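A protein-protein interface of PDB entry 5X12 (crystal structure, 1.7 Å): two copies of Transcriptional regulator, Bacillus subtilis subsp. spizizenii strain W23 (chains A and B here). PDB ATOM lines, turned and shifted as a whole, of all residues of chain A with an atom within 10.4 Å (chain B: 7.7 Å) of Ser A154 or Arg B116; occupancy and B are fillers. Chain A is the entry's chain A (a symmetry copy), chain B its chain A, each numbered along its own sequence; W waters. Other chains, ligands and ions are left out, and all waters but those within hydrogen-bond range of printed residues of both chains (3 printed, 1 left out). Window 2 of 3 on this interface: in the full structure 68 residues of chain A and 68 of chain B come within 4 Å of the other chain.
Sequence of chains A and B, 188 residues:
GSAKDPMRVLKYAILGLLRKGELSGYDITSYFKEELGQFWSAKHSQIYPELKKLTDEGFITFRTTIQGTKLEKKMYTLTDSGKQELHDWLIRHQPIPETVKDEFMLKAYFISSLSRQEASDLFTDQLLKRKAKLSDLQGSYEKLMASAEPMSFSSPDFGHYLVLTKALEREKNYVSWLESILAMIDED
The guanidinium group of Arg B116 lies within salt-bridge range of the side-chain carboxylate of Glu B187 (2.8 Å). The side-chain hydroxyl of Ser B115 sits close to the backbone NH of Gln B117 (3.5 Å). N of Ser B115 sits at hydrogen-bond distance from OE1 of Glu B118 (2.9 Å). The guanidinium group (NH1) of Arg B116 sits at hydrogen-bond distance from the backbone carbonyl oxygen (O) of Ile B185 (2.9 Å). The backbone NH of Ser A154 sits close to the side-chain hydroxyl of Ser A152.
Glu B118 touches His A87. Leu B114 touches Ile A91 (CD2 to CG2, 3.9 Å). Ser B115 touches Phe A153 (C to CZ, 3.97 Å). Arg B116 touches Phe A153. CE1 of Phe A153 touches CB of Ala B119, 3.7 Å away. CB of Phe A153 touches OE2 of Glu B187, 3.9 Å away. Ser A154 touches Arg B116 (OG to NH2, 3.8 Å). Met B184 touches Phe A158. Gly A159 touches Ile B111 (N to CG2, 3.8 Å). Ile B111 touches Leu A162 (CD1 to CD1, 3.7 Å).
Ser A154 touches just one residue of chain B: Arg B116 (3.8 Å). Arg B116 touches just these residues of chain A: Phe A153 and Ser A154. Ser B115 touches one residue of chain A. No residue of chain A comes within 4 Å of Gln B117. Ala B119 touches just one residue of chain A: Phe A153 (3.7 Å). No residue of chain A comes within 4 Å of Ser B120. Of the printed residues of chain B, Phe A153 touches Ser B115 (3.97 Å), Arg B116 (3.5 Å), Ala B119 (3.7 Å), Ile B185 (3.999 Å) and Glu B187 (3.9 Å). Printed residues of chain A within 4 Å of Ser B112: Lys A20 (3.3 Å). Met A151 touches none of the printed residues of chain B. Leu B182 touches none of the printed residues of chain A. The nearest residue of chain B that does not touch Ser A154 is Glu B187 (4.8 Å). The nearest residue of chain A that does not touch Arg B116 is Ser A152 (6.7 Å).
Hydrophobic or aromatic side chains of chain B that line the printed part of chain A: Ile B111, Leu B114, Ala B119, Met B184 and Ile B185. Of the 16 printed residues of chain A, 9 touch a printed residue of chain B. Among the printed residues, 14 pairs touch across the chains. Among the printed residues, no Asp or Glu carboxylate lies within 4 Å of a Lys or Arg side-chain nitrogen of the other chain.
No position is printed for both chains.
Water W1 lies within hydrogen-bond range of the side-chain carboxylate of Glu B118 (2.5 Å), the backbone carbonyl oxygen of Ser B113 (2.7 Å) and a ring nitrogen (ND1) of His A87 (3.4 Å). Water W3 lies within hydrogen-bond range of O of Met B184 (2.7 Å), N of Phe A153 (2.9 Å) and OE2 of Glu B187 (3.3 Å). Water W2 bridges ND1 of His A87 (2.7 Å) and O of Ser B113 (2.9 Å).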
ATOM      1  N   LYS A  20      -2.884  18.047  13.829  1.00  0.00           N
ATOM      2  CA  LYS A  20      -3.674  18.985  14.619  1.00  0.00           C
ATOM      3  C   LYS A  20      -3.233  19.082  16.070  1.00  0.00           C
ATOM      4  O   LYS A  20      -3.835  19.820  16.849  1.00  0.00           O
ATOM      5  CB  LYS A  20      -5.147  18.625  14.540  1.00  0.00           C
ATOM      6  CG  LYS A  20      -5.812  19.178  13.292  1.00  0.00           C
ATOM      7  CD  LYS A  20      -7.300  18.870  13.266  1.00  0.00           C
ATOM      8  CE  LYS A  20      -7.953  19.307  11.961  1.00  0.00           C
ATOM      9  NZ  LYS A  20      -8.647  20.633  12.002  1.00  0.00           N
ATOM     10  N   HIS A  87       3.715  18.280   4.504  1.00  0.00           N
ATOM     11  CA  HIS A  87       3.380  19.285   3.523  1.00  0.00           C
ATOM     12  C   HIS A  87       3.873  18.921   2.132  1.00  0.00           C
ATOM     13  O   HIS A  87       3.116  19.010   1.146  1.00  0.00           O
ATOM     14  CB  HIS A  87       3.910  20.669   3.941  1.00  0.00           C
ATOM     15  CG  HIS A  87       3.601  21.731   2.952  1.00  0.00           C
ATOM     16  ND1 HIS A  87       2.346  22.297   2.874  1.00  0.00           N
ATOM     17  CD2 HIS A  87       4.359  22.336   2.008  1.00  0.00           C
ATOM     18  CE1 HIS A  87       2.334  23.188   1.895  1.00  0.00           C
ATOM     19  NE2 HIS A  87       3.554  23.253   1.369  1.00  0.00           N
ATOM     20  N   ILE A  91       1.430  18.157  -1.222  1.00  0.00           N
ATOM     21  CA  ILE A  91       1.330  18.981  -2.415  1.00  0.00           C
ATOM     22  C   ILE A  91       1.968  18.398  -3.654  1.00  0.00           C
ATOM     23  O   ILE A  91       1.753  18.936  -4.768  1.00  0.00           O
ATOM     24  CB  ILE A  91       1.825  20.415  -2.203  1.00  0.00           C
ATOM     25  CG1 ILE A  91       3.316  20.453  -1.993  1.00  0.00           C
ATOM     26  CG2 ILE A  91       1.010  21.103  -1.085  1.00  0.00           C
ATOM     27  CD1 ILE A  91       3.907  21.871  -2.191  1.00  0.00           C
ATOM     28  N   GLU A 149     -21.856  20.937  13.836  1.00  0.00           N
ATOM     29  CA  GLU A 149     -21.302  21.846  12.825  1.00  0.00           C
ATOM     30  C   GLU A 149     -21.666  21.409  11.393  1.00  0.00           C
ATOM     31  O   GLU A 149     -21.341  20.263  10.993  1.00  0.00           O
ATOM     32  CB  GLU A 149     -19.771  21.900  12.953  1.00  0.00           C
ATOM     33  CG  GLU A 149     -19.111  22.649  11.797  1.00  0.00           C
ATOM     34  CD  GLU A 149     -17.791  23.291  12.143  1.00  0.00           C
ATOM     35  OE1 GLU A 149     -17.307  23.145  13.300  1.00  0.00           O
ATOM     36  OE2 GLU A 149     -17.259  23.967  11.238  1.00  0.00           O
ATOM     37  N   PRO A 150     -22.313  22.313  10.600  1.00  0.00           N
ATOM     38  CA  PRO A 150     -22.668  21.862   9.264  1.00  0.00           C
ATOM     39  C   PRO A 150     -21.396  21.583   8.452  1.00  0.00           C
ATOM     40  O   PRO A 150     -20.312  22.142   8.767  1.00  0.00           O
ATOM     41  CB  PRO A 150     -23.460  23.030   8.653  1.00  0.00           C
ATOM     42  CG  PRO A 150     -23.341  24.122   9.568  1.00  0.00           C
ATOM     43  CD  PRO A 150     -22.851  23.650  10.894  1.00  0.00           C
ATOM     44  N   MET A 151     -21.527  20.744   7.431  1.00  0.00           N
ATOM     45  CA  MET A 151     -20.306  20.321   6.650  1.00  0.00           C
ATOM     46  C   MET A 151     -19.930  21.355   5.602  1.00  0.00           C
ATOM     47  O   MET A 151     -20.761  21.838   4.830  1.00  0.00           O
ATOM     48  CB  MET A 151     -20.534  18.976   5.980  1.00  0.00           C
ATOM     49  CG  MET A 151     -19.340  18.401   5.253  1.00  0.00           C
ATOM     50  SD  MET A 151     -17.882  18.261   6.345  1.00  0.00           S
ATOM     51  CE  MET A 151     -18.481  17.184   7.572  1.00  0.00           C
ATOM     52  N   SER A 152     -18.646  21.648   5.541  1.00  0.00           N
ATOM     53  CA  SER A 152     -18.086  22.546   4.549  1.00  0.00           C
ATOM     54  C   SER A 152     -16.605  22.344   4.566  1.00  0.00           C
ATOM     55  O   SER A 152     -16.062  21.684   5.454  1.00  0.00           O
ATOM     56  CB  SER A 152     -18.424  23.986   4.919  1.00  0.00           C
ATOM     57  OG  SER A 152     -17.628  24.437   5.990  1.00  0.00           O
ATOM     58  N   PHE A 153     -15.932  23.007   3.645  1.00  0.00           N
ATOM     59  CA  PHE A 153     -14.493  22.973   3.586  1.00  0.00           C
ATOM     60  C   PHE A 153     -13.799  23.313   4.915  1.00  0.00           C
ATOM     61  O   PHE A 153     -12.752  22.723   5.249  1.00  0.00           O
ATOM     62  CB  PHE A 153     -14.015  23.925   2.512  1.00  0.00           C
ATOM     63  CG  PHE A 153     -12.534  24.047   2.453  1.00  0.00           C
ATOM     64  CD1 PHE A 153     -11.765  23.035   1.901  1.00  0.00           C
ATOM     65  CD2 PHE A 153     -11.880  25.124   3.006  1.00  0.00           C
ATOM     66  CE1 PHE A 153     -10.372  23.100   1.877  1.00  0.00           C
ATOM     67  CE2 PHE A 153     -10.506  25.203   2.966  1.00  0.00           C
ATOM     68  CZ  PHE A 153      -9.736  24.175   2.380  1.00  0.00           C
ATOM     69  N   SER A 154     -14.389  24.248   5.669  1.00  0.00           N
ATOM     70  CA  SER A 154     -13.817  24.754   6.912  1.00  0.00           C
ATOM     71  C   SER A 154     -14.110  23.882   8.132  1.00  0.00           C
ATOM     72  O   SER A 154     -13.587  24.131   9.242  1.00  0.00           O
ATOM     73  CB  SER A 154     -14.312  26.190   7.168  1.00  0.00           C
ATOM     74  OG  SER A 154     -13.869  27.017   6.133  1.00  0.00           O
ATOM     75  N   SER A 155     -14.937  22.866   7.966  1.00  0.00           N
ATOM     76  CA  SER A 155     -15.239  22.004   9.056  1.00  0.00           C
ATOM     77  C   SER A 155     -14.004  21.196   9.429  1.00  0.00           C
ATOM     78  O   SER A 155     -13.352  20.643   8.559  1.00  0.00           O
ATOM     79  CB  SER A 155     -16.325  21.025   8.658  1.00  0.00           C
ATOM     80  OG  SER A 155     -16.511  20.059   9.694  1.00  0.00           O
ATOM     81  N   PRO A 156     -13.762  20.999  10.722  1.00  0.00           N
ATOM     82  CA  PRO A 156     -12.639  20.125  11.123  1.00  0.00           C
ATOM     83  C   PRO A 156     -12.817  18.687  10.691  1.00  0.00           C
ATOM     84  O   PRO A 156     -11.829  17.948  10.561  1.00  0.00           O
ATOM     85  CB  PRO A 156     -12.647  20.195  12.665  1.00  0.00           C
ATOM     86  CG  PRO A 156     -13.731  21.044  13.029  1.00  0.00           C
ATOM     87  CD  PRO A 156     -14.413  21.651  11.861  1.00  0.00           C
ATOM     88  N   ASP A 157     -14.059  18.278  10.422  1.00  0.00           N
ATOM     89  CA  ASP A 157     -14.349  16.927   9.937  1.00  0.00           C
ATOM     90  C   ASP A 157     -14.379  16.768   8.411  1.00  0.00           C
ATOM     91  O   ASP A 157     -14.788  15.740   7.909  1.00  0.00           O
ATOM     92  CB  ASP A 157     -15.706  16.519  10.503  1.00  0.00           C
ATOM     93  CG  ASP A 157     -15.692  16.387  12.003  1.00  0.00           C
ATOM     94  OD1 ASP A 157     -14.648  16.041  12.595  1.00  0.00           O
ATOM     95  OD2 ASP A 157     -16.759  16.636  12.580  1.00  0.00           O
ATOM     96  N   PHE A 158     -13.945  17.776   7.660  1.00  0.00           N
ATOM     97  CA  PHE A 158     -14.020  17.697   6.208  1.00  0.00           C
ATOM     98  C   PHE A 158     -13.251  16.535   5.634  1.00  0.00           C
ATOM     99  O   PHE A 158     -13.738  15.824   4.760  1.00  0.00           O
ATOM    100  CB  PHE A 158     -13.585  19.022   5.581  1.00  0.00           C
ATOM    101  CG  PHE A 158     -13.914  19.163   4.095  1.00  0.00           C
ATOM    102  CD1 PHE A 158     -15.214  19.019   3.633  1.00  0.00           C
ATOM    103  CD2 PHE A 158     -12.944  19.517   3.185  1.00  0.00           C
ATOM    104  CE1 PHE A 158     -15.484  19.151   2.262  1.00  0.00           C
ATOM    105  CE2 PHE A 158     -13.241  19.683   1.822  1.00  0.00           C
ATOM    106  CZ  PHE A 158     -14.504  19.511   1.389  1.00  0.00           C
ATOM    107  N   GLY A 159     -12.031  16.311   6.114  1.00  0.00           N
ATOM    108  CA  GLY A 159     -11.270  15.167   5.647  1.00  0.00           C
ATOM    109  C   GLY A 159     -11.969  13.833   5.805  1.00  0.00           C
ATOM    110  O   GLY A 159     -11.948  12.983   4.931  1.00  0.00           O
ATOM    111  N   TYR A 161     -15.178  13.415   6.118  1.00  0.00           N
ATOM    112  CA  TYR A 161     -16.266  13.476   5.127  1.00  0.00           C
ATOM    113  C   TYR A 161     -15.843  13.085   3.735  1.00  0.00           C
ATOM    114  O   TYR A 161     -16.531  12.385   2.997  1.00  0.00           O
ATOM    115  CB  TYR A 161     -16.870  14.881   5.149  1.00  0.00           C
ATOM    116  CG  TYR A 161     -17.912  15.145   4.120  1.00  0.00           C
ATOM    117  CD1 TYR A 161     -19.228  14.855   4.365  1.00  0.00           C
ATOM    118  CD2 TYR A 161     -17.589  15.762   2.892  1.00  0.00           C
ATOM    119  CE1 TYR A 161     -20.242  15.115   3.425  1.00  0.00           C
ATOM    120  CE2 TYR A 161     -18.588  16.022   1.942  1.00  0.00           C
ATOM    121  CZ  TYR A 161     -19.883  15.730   2.224  1.00  0.00           C
ATOM    122  OH  TYR A 161     -20.882  15.966   1.286  1.00  0.00           O
ATOM    123  N   LEU A 162     -14.657  13.533   3.332  1.00  0.00           N
ATOM    124  CA  LEU A 162     -14.105  13.183   2.030  1.00  0.00           C
ATOM    125  C   LEU A 162     -13.886  11.686   1.886  1.00  0.00           C
ATOM    126  O   LEU A 162     -14.357  11.092   0.909  1.00  0.00           O
ATOM    127  CB  LEU A 162     -12.770  13.942   1.743  1.00  0.00           C
ATOM    128  CG  LEU A 162     -12.960  15.452   1.617  1.00  0.00           C
ATOM    129  CD1 LEU A 162     -11.582  16.105   1.249  1.00  0.00           C
ATOM    130  CD2 LEU A 162     -14.074  15.901   0.636  1.00  0.00           C
ATOM    131  N   ILE B 111      -6.676  16.885   4.587  1.00  0.00           N
ATOM    132  CA  ILE B 111      -6.891  18.168   3.897  1.00  0.00           C
ATOM    133  C   ILE B 111      -6.812  19.408   4.796  1.00  0.00           C
ATOM    134  O   ILE B 111      -6.535  20.529   4.320  1.00  0.00           O
ATOM    135  CB  ILE B 111      -8.253  18.165   3.134  1.00  0.00           C
ATOM    136  CG1 ILE B 111      -8.310  19.306   2.101  1.00  0.00           C
ATOM    137  CG2 ILE B 111      -9.458  18.197   4.136  1.00  0.00           C
ATOM    138  CD1 ILE B 111      -9.487  19.179   1.093  1.00  0.00           C
ATOM    139  N   SER B 112      -7.036  19.259   6.092  1.00  0.00           N
ATOM    140  CA  SER B 112      -6.989  20.421   6.997  1.00  0.00           C
ATOM    141  C   SER B 112      -5.586  21.062   7.005  1.00  0.00           C
ATOM    142  O   SER B 112      -5.463  22.225   7.416  1.00  0.00           O
ATOM    143  CB  SER B 112      -7.336  20.062   8.448  1.00  0.00           C
ATOM    144  OG  SER B 112      -6.362  19.162   9.018  1.00  0.00           O
ATOM    145  N   SER B 113      -4.551  20.321   6.569  1.00  0.00           N
ATOM    146  CA  SER B 113      -3.205  20.842   6.475  1.00  0.00           C
ATOM    147  C   SER B 113      -2.942  21.711   5.235  1.00  0.00           C
ATOM    148  O   SER B 113      -1.855  22.284   5.108  1.00  0.00           O
ATOM    149  CB  SER B 113      -2.191  19.709   6.542  1.00  0.00           C
ATOM    150  OG  SER B 113      -2.085  19.197   7.863  1.00  0.00           O
ATOM    151  N   LEU B 114      -3.941  21.828   4.342  1.00  0.00           N
ATOM    152  CA  LEU B 114      -3.858  22.634   3.107  1.00  0.00           C
ATOM    153  C   LEU B 114      -4.779  23.848   3.160  1.00  0.00           C
ATOM    154  O   LEU B 114      -5.881  23.797   3.738  1.00  0.00           O
ATOM    155  CB  LEU B 114      -4.236  21.765   1.894  1.00  0.00           C
ATOM    156  CG  LEU B 114      -3.313  20.589   1.641  1.00  0.00           C
ATOM    157  CD1 LEU B 114      -3.812  19.851   0.372  1.00  0.00           C
ATOM    158  CD2 LEU B 114      -1.832  20.949   1.555  1.00  0.00           C
ATOM    159  N   SER B 115      -4.330  24.959   2.555  1.00  0.00           N
ATOM    160  CA  SER B 115      -5.174  26.085   2.408  1.00  0.00           C
ATOM    161  C   SER B 115      -6.253  25.766   1.351  1.00  0.00           C
ATOM    162  O   SER B 115      -6.114  24.817   0.629  1.00  0.00           O
ATOM    163  CB  SER B 115      -4.400  27.291   1.927  1.00  0.00           C
ATOM    164  OG  SER B 115      -3.950  27.121   0.602  1.00  0.00           O
ATOM    165  N   ARG B 116      -7.217  26.654   1.229  1.00  0.00           N
ATOM    166  CA  ARG B 116      -8.282  26.463   0.236  1.00  0.00           C
ATOM    167  C   ARG B 116      -7.683  26.409  -1.145  1.00  0.00           C
ATOM    168  O   ARG B 116      -8.078  25.565  -1.958  1.00  0.00           O
ATOM    169  CB  ARG B 116      -9.313  27.570   0.343  1.00  0.00           C
ATOM    170  CG  ARG B 116     -10.582  27.327  -0.473  1.00  0.00           C
ATOM    171  CD  ARG B 116     -11.585  28.498  -0.409  1.00  0.00           C
ATOM    172  NE  ARG B 116     -12.174  28.787   0.925  1.00  0.00           N
ATOM    173  CZ  ARG B 116     -13.230  28.219   1.487  1.00  0.00           C
ATOM    174  NH1 ARG B 116     -13.953  27.303   0.864  1.00  0.00           N
ATOM    175  NH2 ARG B 116     -13.609  28.630   2.711  1.00  0.00           N
ATOM    176  N   GLN B 117      -6.726  27.301  -1.453  1.00  0.00           N
ATOM    177  CA  GLN B 117      -6.110  27.268  -2.750  1.00  0.00           C
ATOM    178  C   GLN B 117      -5.274  25.999  -2.994  1.00  0.00           C
ATOM    179  O   GLN B 117      -5.306  25.446  -4.094  1.00  0.00           O
ATOM    180  CB  GLN B 117      -5.271  28.532  -3.040  1.00  0.00           C
ATOM    181  CG  GLN B 117      -4.728  28.591  -4.488  1.00  0.00           C
ATOM    182  CD  GLN B 117      -5.875  28.654  -5.509  1.00  0.00           C
ATOM    183  OE1 GLN B 117      -6.758  29.515  -5.396  1.00  0.00           O
ATOM    184  NE2 GLN B 117      -5.898  27.720  -6.459  1.00  0.00           N
ATOM    185  N   GLU B 118      -4.533  25.560  -1.991  1.00  0.00           N
ATOM    186  CA  GLU B 118      -3.712  24.356  -2.140  1.00  0.00           C
ATOM    187  C   GLU B 118      -4.618  23.156  -2.331  1.00  0.00           C
ATOM    188  O   GLU B 118      -4.294  22.260  -3.137  1.00  0.00           O
ATOM    189  CB  GLU B 118      -2.798  24.130  -0.927  1.00  0.00           C
ATOM    190  CG  GLU B 118      -1.679  25.110  -0.791  1.00  0.00           C
ATOM    191  CD  GLU B 118      -0.937  25.023   0.541  1.00  0.00           C
ATOM    192  OE1 GLU B 118      -1.558  24.722   1.599  1.00  0.00           O
ATOM    193  OE2 GLU B 118       0.274  25.305   0.528  1.00  0.00           O
ATOM    194  N   ALA B 119      -5.739  23.133  -1.618  1.00  0.00           N
ATOM    195  CA  ALA B 119      -6.709  22.015  -1.721  1.00  0.00           C
ATOM    196  C   ALA B 119      -7.282  22.007  -3.140  1.00  0.00           C
ATOM    197  O   ALA B 119      -7.360  20.962  -3.815  1.00  0.00           O
ATOM    198  CB  ALA B 119      -7.798  22.123  -0.633  1.00  0.00           C
ATOM    199  N   SER B 120      -7.670  23.182  -3.613  1.00  0.00           N
ATOM    200  CA  SER B 120      -8.184  23.301  -4.972  1.00  0.00           C
ATOM    201  C   SER B 120      -7.156  22.809  -5.990  1.00  0.00           C
ATOM    202  O   SER B 120      -7.475  22.066  -6.904  1.00  0.00           O
ATOM    203  CB  SER B 120      -8.540  24.736  -5.265  1.00  0.00           C
ATOM    204  OG  SER B 120      -9.180  24.799  -6.544  1.00  0.00           O
ATOM    205  N   ASP B 121      -5.885  23.169  -5.795  1.00  0.00           N
ATOM    206  CA  ASP B 121      -4.829  22.790  -6.762  1.00  0.00           C
ATOM    207  C   ASP B 121      -4.599  21.257  -6.756  1.00  0.00           C
ATOM    208  O   ASP B 121      -4.443  20.642  -7.793  1.00  0.00           O
ATOM    209  CB  ASP B 121      -3.538  23.563  -6.494  1.00  0.00           C
ATOM    210  CG  ASP B 121      -3.630  25.047  -6.862  1.00  0.00           C
ATOM    211  OD1 ASP B 121      -4.617  25.534  -7.476  1.00  0.00           O
ATOM    212  OD2 ASP B 121      -2.697  25.768  -6.478  1.00  0.00           O
ATOM    213  N   LEU B 122      -4.598  20.686  -5.567  1.00  0.00           N
ATOM    214  CA  LEU B 122      -4.430  19.219  -5.394  1.00  0.00           C
ATOM    215  C   LEU B 122      -5.550  18.432  -6.066  1.00  0.00           C
ATOM    216  O   LEU B 122      -5.307  17.525  -6.857  1.00  0.00           O
ATOM    217  CB  LEU B 122      -4.300  18.873  -3.932  1.00  0.00           C
ATOM    218  CG  LEU B 122      -4.273  17.369  -3.588  1.00  0.00           C
ATOM    219  CD1 LEU B 122      -3.061  16.771  -4.233  1.00  0.00           C
ATOM    220  CD2 LEU B 122      -4.433  17.140  -2.040  1.00  0.00           C
ATOM    221  N   LEU B 182     -14.478  19.774  -5.585  1.00  0.00           N
ATOM    222  CA  LEU B 182     -13.937  21.041  -6.026  1.00  0.00           C
ATOM    223  C   LEU B 182     -14.991  22.138  -5.866  1.00  0.00           C
ATOM    224  O   LEU B 182     -14.668  23.263  -5.539  1.00  0.00           O
ATOM    225  CB  LEU B 182     -13.498  20.976  -7.498  1.00  0.00           C
ATOM    226  CG  LEU B 182     -12.139  20.315  -7.709  1.00  0.00           C
ATOM    227  CD1 LEU B 182     -11.965  19.888  -9.197  1.00  0.00           C
ATOM    228  CD2 LEU B 182     -10.973  21.276  -7.274  1.00  0.00           C
ATOM    229  N   ALA B 183     -16.264  21.809  -6.076  1.00  0.00           N
ATOM    230  CA  ALA B 183     -17.298  22.802  -5.914  1.00  0.00           C
ATOM    231  C   ALA B 183     -17.455  23.181  -4.422  1.00  0.00           C
ATOM    232  O   ALA B 183     -17.759  24.325  -4.105  1.00  0.00           O
ATOM    233  CB  ALA B 183     -18.663  22.245  -6.486  1.00  0.00           C
ATOM    234  N   MET B 184     -17.266  22.235  -3.530  1.00  0.00           N
ATOM    235  CA  MET B 184     -17.217  22.532  -2.070  1.00  0.00           C
ATOM    236  C   MET B 184     -16.025  23.398  -1.672  1.00  0.00           C
ATOM    237  O   MET B 184     -16.166  24.316  -0.870  1.00  0.00           O
ATOM    238  CB  MET B 184     -17.260  21.254  -1.219  1.00  0.00           C
ATOM    239  CG  MET B 184     -18.530  20.523  -1.397  1.00  0.00           C
ATOM    240  SD  MET B 184     -18.568  19.103  -0.257  1.00  0.00           S
ATOM    241  CE  MET B 184     -19.003  19.862   1.314  1.00  0.00           C
ATOM    242  N   ILE B 185     -14.848  23.102  -2.201  1.00  0.00           N
ATOM    243  CA  ILE B 185     -13.645  23.883  -1.957  1.00  0.00           C
ATOM    244  C   ILE B 185     -13.891  25.321  -2.483  1.00  0.00           C
ATOM    245  O   ILE B 185     -13.531  26.305  -1.802  1.00  0.00           O
ATOM    246  CB  ILE B 185     -12.450  23.255  -2.614  1.00  0.00           C
ATOM    247  CG1 ILE B 185     -12.104  21.934  -1.928  1.00  0.00           C
ATOM    248  CG2 ILE B 185     -11.183  24.170  -2.503  1.00  0.00           C
ATOM    249  CD1 ILE B 185     -11.132  21.095  -2.658  1.00  0.00           C
ATOM    250  N   ASP B 186     -14.598  25.436  -3.629  1.00  0.00           N
ATOM    251  CA  ASP B 186     -14.933  26.728  -4.253  1.00  0.00           C
ATOM    252  C   ASP B 186     -16.343  27.202  -3.928  1.00  0.00           C
ATOM    253  O   ASP B 186     -17.099  27.620  -4.813  1.00  0.00           O
ATOM    254  CB  ASP B 186     -14.827  26.581  -5.772  1.00  0.00           C
ATOM    255  CG  ASP B 186     -14.888  27.892  -6.523  1.00  0.00           C
ATOM    256  OD1 ASP B 186     -14.491  28.923  -5.961  1.00  0.00           O
ATOM    257  OD2 ASP B 186     -15.283  27.827  -7.720  1.00  0.00           O
ATOM    258  N   GLU B 187     -16.745  27.014  -2.687  1.00  0.00           N
ATOM    259  CA  GLU B 187     -18.112  27.287  -2.313  1.00  0.00           C
ATOM    260  C   GLU B 187     -18.480  28.753  -2.525  1.00  0.00           C
ATOM    261  O   GLU B 187     -17.636  29.622  -2.390  1.00  0.00           O
ATOM    262  CB  GLU B 187     -18.284  26.916  -0.852  1.00  0.00           C
ATOM    263  CG  GLU B 187     -17.429  27.771   0.091  1.00  0.00           C
ATOM    264  CD  GLU B 187     -17.536  27.308   1.534  1.00  0.00           C
ATOM    265  OE1 GLU B 187     -18.708  27.336   2.034  1.00  0.00           O
ATOM    266  OE2 GLU B 187     -16.468  26.935   2.148  1.00  0.00           O
ATOM    267  N   ASP B 188     -19.738  29.009  -2.875  1.00  0.00           N
ATOM    268  CA  ASP B 188     -20.244  30.369  -3.093  1.00  0.00           C
ATOM    269  C   ASP B 188     -20.003  31.235  -1.853  1.00  0.00           C
ATOM    270  O   ASP B 188     -20.074  30.695  -0.743  1.00  0.00           O
ATOM    271  CB  ASP B 188     -21.747  30.323  -3.364  1.00  0.00           C
ATOM    272  CG  ASP B 188     -22.110  29.835  -4.755  1.00  0.00           C
ATOM    273  OD1 ASP B 188     -21.230  29.545  -5.567  1.00  0.00           O
ATOM    274  OD2 ASP B 188     -23.321  29.731  -5.029  1.00  0.00           O
ATOM    275  OXT ASP B 188     -19.813  32.456  -1.910  1.00  0.00           O
HETATM  276  O   HOH W   1      -0.368  24.104   3.723  1.00  0.00           O
HETATM  277  O   HOH W   2       0.782  21.152   4.809  1.00  0.00           O
HETATM  278  O   HOH W   3     -17.556  23.954   1.383  1.00  0.00           O
